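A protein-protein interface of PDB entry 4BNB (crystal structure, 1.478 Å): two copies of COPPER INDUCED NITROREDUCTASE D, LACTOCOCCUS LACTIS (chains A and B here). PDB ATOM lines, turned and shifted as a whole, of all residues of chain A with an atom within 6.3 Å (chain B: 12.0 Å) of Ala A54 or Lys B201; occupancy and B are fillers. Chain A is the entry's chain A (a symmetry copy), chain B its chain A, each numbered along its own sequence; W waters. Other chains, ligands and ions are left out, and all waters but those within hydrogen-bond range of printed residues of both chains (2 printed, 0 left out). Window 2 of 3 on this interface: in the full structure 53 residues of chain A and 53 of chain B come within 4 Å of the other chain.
The backbone carbonyl oxygen (O) of Ile B198 is in hydrogen-bond range of the backbone NH (N) of Ile A49 (2.8 Å).
The backbone carbonyl oxygen (O) of Ala B200 sits at hydrogen-bond distance from the backbone NH (N) of Thr A51 (3.2 Å).
O of Ile A49 lies within hydrogen-bond range of N of Ala B200 (2.9 Å).
Of the printed residues of chain B, Ile A49 touches Ile B198, Val B199 and Ala B200.
Printed residues of chain B within 4 Å of Leu A50: Ala B200.
Of chain B, only Ala B200 and Lys B201 come within 4 Å of Thr A51.
No residue of chain B comes within 4 Å of Asp A53.
Of the printed residues of chain B, Ala A54 touches Ala B200 (3.9 Å) and Lys B201 (3.6 Å).
No residue of chain B comes within 4 Å of Gln A55.
No residue of chain B comes within 4 Å of Lys A57.
Trp A59 touches none of the printed residues of chain B.
Of the printed residues of chain B, Trp A164 touches Ala B200.
Printed residues of chain A within 4 Å of Ile B198: Ile A49.
Of the printed residues of chain A, Val B199 touches Ile A49 (3.5 Å).
Printed residues of chain A within 4 Å of Ala B200: Ile A49 (2.9 Å), Leu A50 (3.5 Å), Thr A51 (3.2 Å), Ala A54 (3.9 Å) and Trp A164 (3.7 Å).
Lys B201 touches two residues of chain A.
The nearest residue of chain B that does not touch Ala A54 is Val B199 (7.2 Å).
Water W1 bridges the side-chain hydroxyl (OG1) of Thr A51 (2.8 Å) and the backbone carbonyl oxygen (O) of Ala B200 (2.9 Å).
Water W2 bridges NE1 of Trp A164 and O of Lys B201.
Of the 5 printed residues of chain B, 4 touch a printed residue of chain A.
Printed residues of chain B that touch a printed residue of chain A: Ile B198, Val B199, Ala B200 and Lys B201.
Along chain B the printed residues that touch a printed residue of chain A span positions 198 to 201.
Of the 14 printed residues of chain A, 5 touch a printed residue of chain B.
Among the printed residues, 9 pairs touch across the chains.
Among the printed residues, no Asp or Glu carboxylate lies within 4 Å of a Lys or Arg side-chain nitrogen of the other chain.
Among the printed residues, merely in contact across the chains: Ile A49 with Val B199, Leu A50 with Ala B200, Thr A51 with Lys B201, Ala A54 with Ala B200, Ala A54 with Lys B201 and Trp A164 with Ala B200.
No position is printed for both chains.
Of the 9 pairs that touch across the chains among the printed residues, none has its exchanged pair printed and touching as well.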
ATOM      1  N   GLU A  22     -21.993 -22.156 -12.133  1.00  0.00           N
ATOM      2  CA  GLU A  22     -21.055 -21.118 -11.728  1.00  0.00           C
ATOM      3  C   GLU A  22     -21.789 -19.834 -11.350  1.00  0.00           C
ATOM      4  O   GLU A  22     -21.383 -19.120 -10.434  1.00  0.00           O
ATOM      5  CB  GLU A  22     -20.071 -20.819 -12.856  1.00  0.00           C
ATOM      6  CG  GLU A  22     -19.485 -22.046 -13.536  1.00  0.00           C
ATOM      7  CD  GLU A  22     -18.984 -21.749 -14.940  1.00  0.00           C
ATOM      8  OE1 GLU A  22     -19.758 -21.171 -15.733  1.00  0.00           O
ATOM      9  OE2 GLU A  22     -17.825 -22.095 -15.253  1.00  0.00           O
ATOM     10  N   ILE A  26     -21.451 -17.662  -7.846  1.00  0.00           N
ATOM     11  CA  ILE A  26     -21.165 -16.231  -7.768  1.00  0.00           C
ATOM     12  C   ILE A  26     -22.236 -15.494  -6.957  1.00  0.00           C
ATOM     13  O   ILE A  26     -21.917 -14.660  -6.103  1.00  0.00           O
ATOM     14  CB  ILE A  26     -21.065 -15.599  -9.175  1.00  0.00           C
ATOM     15  CG1 ILE A  26     -19.912 -16.221  -9.964  1.00  0.00           C
ATOM     16  CG2 ILE A  26     -20.870 -14.094  -9.080  1.00  0.00           C
ATOM     17  CD1 ILE A  26     -18.561 -16.081  -9.302  1.00  0.00           C
ATOM     18  N   ILE A  49     -12.972 -12.244  -7.632  1.00  0.00           N
ATOM     19  CA  ILE A  49     -13.330 -13.645  -7.813  1.00  0.00           C
ATOM     20  C   ILE A  49     -12.793 -14.133  -9.149  1.00  0.00           C
ATOM     21  O   ILE A  49     -13.212 -13.649 -10.201  1.00  0.00           O
ATOM     22  CB  ILE A  49     -14.860 -13.824  -7.778  1.00  0.00           C
ATOM     23  CG1 ILE A  49     -15.422 -13.318  -6.445  1.00  0.00           C
ATOM     24  CG2 ILE A  49     -15.238 -15.282  -7.991  1.00  0.00           C
ATOM     25  CD1 ILE A  49     -16.920 -13.081  -6.459  1.00  0.00           C
ATOM     26  N   LEU A  50     -11.864 -15.083  -9.106  1.00  0.00           N
ATOM     27  CA  LEU A  50     -11.205 -15.572 -10.314  1.00  0.00           C
ATOM     28  C   LEU A  50     -11.557 -17.025 -10.610  1.00  0.00           C
ATOM     29  O   LEU A  50     -11.520 -17.873  -9.724  1.00  0.00           O
ATOM     30  CB  LEU A  50      -9.685 -15.455 -10.176  1.00  0.00           C
ATOM     31  CG  LEU A  50      -9.110 -14.091  -9.792  1.00  0.00           C
ATOM     32  CD1 LEU A  50      -7.595 -14.188  -9.694  1.00  0.00           C
ATOM     33  CD2 LEU A  50      -9.517 -13.014 -10.784  1.00  0.00           C
ATOM     34  N   THR A  51     -11.886 -17.302 -11.869  1.00  0.00           N
ATOM     35  CA  THR A  51     -12.099 -18.666 -12.338  1.00  0.00           C
ATOM     36  C   THR A  51     -11.473 -18.825 -13.720  1.00  0.00           C
ATOM     37  O   THR A  51     -11.020 -17.851 -14.318  1.00  0.00           O
ATOM     38  CB  THR A  51     -13.600 -19.017 -12.421  1.00  0.00           C
ATOM     39  OG1 THR A  51     -14.219 -18.259 -13.467  1.00  0.00           O
ATOM     40  CG2 THR A  51     -14.298 -18.721 -11.108  1.00  0.00           C
ATOM     41  N   GLY A  52     -11.441 -20.054 -14.222  1.00  0.00           N
ATOM     42  CA  GLY A  52     -10.952 -20.315 -15.566  1.00  0.00           C
ATOM     43  C   GLY A  52      -9.537 -19.820 -15.805  1.00  0.00           C
ATOM     44  O   GLY A  52      -8.633 -20.089 -15.017  1.00  0.00           O
ATOM     45  N   ASP A  53      -9.344 -19.097 -16.904  1.00  0.00           N
ATOM     46  CA  ASP A  53      -8.018 -18.615 -17.279  1.00  0.00           C
ATOM     47  C   ASP A  53      -7.388 -17.749 -16.196  1.00  0.00           C
ATOM     48  O   ASP A  53      -6.173 -17.782 -16.002  1.00  0.00           O
ATOM     49  CB  ASP A  53      -8.086 -17.826 -18.587  1.00  0.00           C
ATOM     50  CG  ASP A  53      -8.427 -18.694 -19.777  1.00  0.00           C
ATOM     51  OD1 ASP A  53      -8.403 -19.934 -19.639  1.00  0.00           O
ATOM     52  OD2 ASP A  53      -8.709 -18.135 -20.857  1.00  0.00           O
ATOM     53  N   ALA A  54      -8.209 -16.971 -15.496  1.00  0.00           N
ATOM     54  CA  ALA A  54      -7.708 -16.080 -14.455  1.00  0.00           C
ATOM     55  C   ALA A  54      -7.204 -16.884 -13.261  1.00  0.00           C
ATOM     56  O   ALA A  54      -6.219 -16.516 -12.622  1.00  0.00           O
ATOM     57  CB  ALA A  54      -8.792 -15.107 -14.019  1.00  0.00           C
ATOM     58  N   GLN A  55      -7.893 -17.979 -12.964  1.00  0.00           N
ATOM     59  CA  GLN A  55      -7.475 -18.895 -11.910  1.00  0.00           C
ATOM     60  C   GLN A  55      -6.112 -19.505 -12.258  1.00  0.00           C
ATOM     61  O   GLN A  55      -5.214 -19.553 -11.419  1.00  0.00           O
ATOM     62  CB  GLN A  55      -8.547 -19.977 -11.711  1.00  0.00           C
ATOM     63  CG  GLN A  55      -8.093 -21.245 -10.991  1.00  0.00           C
ATOM     64  CD  GLN A  55      -7.843 -21.043  -9.511  1.00  0.00           C
ATOM     65  OE1 GLN A  55      -7.968 -19.938  -8.989  1.00  0.00           O
ATOM     66  NE2 GLN A  55      -7.491 -22.122  -8.823  1.00  0.00           N
ATOM     67  N   ASP A  56      -5.948 -19.949 -13.502  1.00  0.00           N
ATOM     68  CA  ASP A  56      -4.660 -20.466 -13.948  1.00  0.00           C
ATOM     69  C   ASP A  56      -3.579 -19.393 -13.823  1.00  0.00           C
ATOM     70  O   ASP A  56      -2.472 -19.662 -13.358  1.00  0.00           O
ATOM     71  CB  ASP A  56      -4.739 -20.935 -15.402  1.00  0.00           C
ATOM     72  CG  ASP A  56      -5.625 -22.153 -15.580  1.00  0.00           C
ATOM     73  OD1 ASP A  56      -5.901 -22.847 -14.581  1.00  0.00           O
ATOM     74  OD2 ASP A  56      -6.031 -22.424 -16.732  1.00  0.00           O
ATOM     75  N   LYS A  57      -3.909 -18.176 -14.238  1.00  0.00           N
ATOM     76  CA  LYS A  57      -2.937 -17.089 -14.262  1.00  0.00           C
ATOM     77  C   LYS A  57      -2.450 -16.725 -12.864  1.00  0.00           C
ATOM     78  O   LYS A  57      -1.258 -16.512 -12.651  1.00  0.00           O
ATOM     79  CB  LYS A  57      -3.528 -15.855 -14.946  1.00  0.00           C
ATOM     80  CG  LYS A  57      -2.577 -14.665 -14.968  1.00  0.00           C
ATOM     81  CD  LYS A  57      -3.116 -13.508 -15.796  1.00  0.00           C
ATOM     82  CE  LYS A  57      -3.144 -13.844 -17.276  1.00  0.00           C
ATOM     83  NZ  LYS A  57      -3.496 -12.662 -18.109  1.00  0.00           N
ATOM     84  N   LEU A  58      -3.372 -16.650 -11.910  1.00  0.00           N
ATOM     85  CA  LEU A  58      -3.004 -16.285 -10.550  1.00  0.00           C
ATOM     86  C   LEU A  58      -1.892 -17.194 -10.046  1.00  0.00           C
ATOM     87  O   LEU A  58      -0.858 -16.727  -9.574  1.00  0.00           O
ATOM     88  CB  LEU A  58      -4.212 -16.376  -9.615  1.00  0.00           C
ATOM     89  CG  LEU A  58      -3.903 -16.151  -8.130  1.00  0.00           C
ATOM     90  CD1 LEU A  58      -3.310 -14.766  -7.904  1.00  0.00           C
ATOM     91  CD2 LEU A  58      -5.145 -16.347  -7.272  1.00  0.00           C
ATOM     92  N   TRP A  59      -2.104 -18.498 -10.156  1.00  0.00           N
ATOM     93  CA  TRP A  59      -1.204 -19.458  -9.534  1.00  0.00           C
ATOM     94  C   TRP A  59       0.065 -19.718 -10.345  1.00  0.00           C
ATOM     95  O   TRP A  59       1.148 -19.830  -9.775  1.00  0.00           O
ATOM     96  CB  TRP A  59      -1.965 -20.748  -9.220  1.00  0.00           C
ATOM     97  CG  TRP A  59      -2.998 -20.487  -8.169  1.00  0.00           C
ATOM     98  CD1 TRP A  59      -4.336 -20.287  -8.357  1.00  0.00           C
ATOM     99  CD2 TRP A  59      -2.763 -20.345  -6.765  1.00  0.00           C
ATOM    100  NE1 TRP A  59      -4.949 -20.042  -7.151  1.00  0.00           N
ATOM    101  CE2 TRP A  59      -4.004 -20.074  -6.159  1.00  0.00           C
ATOM    102  CE3 TRP A  59      -1.622 -20.428  -5.961  1.00  0.00           C
ATOM    103  CZ2 TRP A  59      -4.136 -19.887  -4.786  1.00  0.00           C
ATOM    104  CZ3 TRP A  59      -1.756 -20.246  -4.599  1.00  0.00           C
ATOM    105  CH2 TRP A  59      -3.003 -19.979  -4.025  1.00  0.00           C
ATOM    106  N   TRP A 164      -5.346  -7.155 -12.474  1.00  0.00           N
ATOM    107  CA  TRP A 164      -6.792  -6.952 -12.493  1.00  0.00           C
ATOM    108  C   TRP A 164      -7.183  -5.505 -12.178  1.00  0.00           C
ATOM    109  O   TRP A 164      -8.340  -5.213 -11.866  1.00  0.00           O
ATOM    110  CB  TRP A 164      -7.479  -7.966 -11.568  1.00  0.00           C
ATOM    111  CG  TRP A 164      -7.390  -9.347 -12.155  1.00  0.00           C
ATOM    112  CD1 TRP A 164      -8.166  -9.858 -13.151  1.00  0.00           C
ATOM    113  CD2 TRP A 164      -6.446 -10.372 -11.817  1.00  0.00           C
ATOM    114  NE1 TRP A 164      -7.773 -11.138 -13.450  1.00  0.00           N
ATOM    115  CE2 TRP A 164      -6.718 -11.478 -12.646  1.00  0.00           C
ATOM    116  CE3 TRP A 164      -5.401 -10.463 -10.893  1.00  0.00           C
ATOM    117  CZ2 TRP A 164      -5.987 -12.663 -12.575  1.00  0.00           C
ATOM    118  CZ3 TRP A 164      -4.676 -11.642 -10.824  1.00  0.00           C
ATOM    119  CH2 TRP A 164      -4.972 -12.725 -11.661  1.00  0.00           C
ATOM    120  N   PHE B 197     -17.436  -6.047  -5.732  1.00  0.00           N
ATOM    121  CA  PHE B 197     -17.216  -7.354  -6.349  1.00  0.00           C
ATOM    122  C   PHE B 197     -16.704  -7.216  -7.777  1.00  0.00           C
ATOM    123  O   PHE B 197     -17.322  -6.554  -8.610  1.00  0.00           O
ATOM    124  CB  PHE B 197     -18.496  -8.200  -6.381  1.00  0.00           C
ATOM    125  CG  PHE B 197     -19.192  -8.323  -5.054  1.00  0.00           C
ATOM    126  CD1 PHE B 197     -18.619  -9.031  -4.015  1.00  0.00           C
ATOM    127  CD2 PHE B 197     -20.438  -7.754  -4.863  1.00  0.00           C
ATOM    128  CE1 PHE B 197     -19.266  -9.151  -2.802  1.00  0.00           C
ATOM    129  CE2 PHE B 197     -21.090  -7.870  -3.653  1.00  0.00           C
ATOM    130  CZ  PHE B 197     -20.505  -8.569  -2.621  1.00  0.00           C
ATOM    131  N   ILE B 198     -15.569  -7.851  -8.048  1.00  0.00           N
ATOM    132  CA  ILE B 198     -15.052  -7.971  -9.402  1.00  0.00           C
ATOM    133  C   ILE B 198     -14.941  -9.452  -9.737  1.00  0.00           C
ATOM    134  O   ILE B 198     -14.339 -10.222  -8.987  1.00  0.00           O
ATOM    135  CB  ILE B 198     -13.665  -7.330  -9.548  1.00  0.00           C
ATOM    136  CG1 ILE B 198     -13.733  -5.833  -9.240  1.00  0.00           C
ATOM    137  CG2 ILE B 198     -13.124  -7.557 -10.955  1.00  0.00           C
ATOM    138  CD1 ILE B 198     -12.377  -5.167  -9.153  1.00  0.00           C
ATOM    139  N   VAL B 199     -15.533  -9.845 -10.856  1.00  0.00           N
ATOM    140  CA  VAL B 199     -15.466 -11.223 -11.317  1.00  0.00           C
ATOM    141  C   VAL B 199     -14.688 -11.274 -12.626  1.00  0.00           C
ATOM    142  O   VAL B 199     -15.018 -10.570 -13.578  1.00  0.00           O
ATOM    143  CB  VAL B 199     -16.872 -11.810 -11.529  1.00  0.00           C
ATOM    144  CG1 VAL B 199     -16.785 -13.244 -12.032  1.00  0.00           C
ATOM    145  CG2 VAL B 199     -17.673 -11.742 -10.240  1.00  0.00           C
ATOM    146  N   ALA B 200     -13.646 -12.101 -12.661  1.00  0.00           N
ATOM    147  CA  ALA B 200     -12.802 -12.222 -13.845  1.00  0.00           C
ATOM    148  C   ALA B 200     -12.575 -13.685 -14.210  1.00  0.00           C
ATOM    149  O   ALA B 200     -12.561 -14.560 -13.341  1.00  0.00           O
ATOM    150  CB  ALA B 200     -11.471 -11.525 -13.617  1.00  0.00           C
ATOM    151  N   LYS B 201     -12.388 -13.943 -15.501  1.00  0.00           N
ATOM    152  CA  LYS B 201     -12.169 -15.297 -15.992  1.00  0.00           C
ATOM    153  C   LYS B 201     -11.019 -15.330 -16.994  1.00  0.00           C
ATOM    154  O   LYS B 201     -10.534 -14.285 -17.432  1.00  0.00           O
ATOM    155  CB  LYS B 201     -13.445 -15.840 -16.639  1.00  0.00           C
ATOM    156  CG  LYS B 201     -14.684 -15.656 -15.779  1.00  0.00           C
ATOM    157  CD  LYS B 201     -15.870 -16.449 -16.302  1.00  0.00           C
ATOM    158  CE  LYS B 201     -17.076 -16.292 -15.386  1.00  0.00           C
ATOM    159  NZ  LYS B 201     -18.201 -17.195 -15.756  1.00  0.00           N
HETATM  160  O   HOH W   1     -15.052 -15.717 -12.556  1.00  0.00           O
HETATM  161  O   HOH W   2      -8.601 -12.066 -16.155  1.00  0.00           O
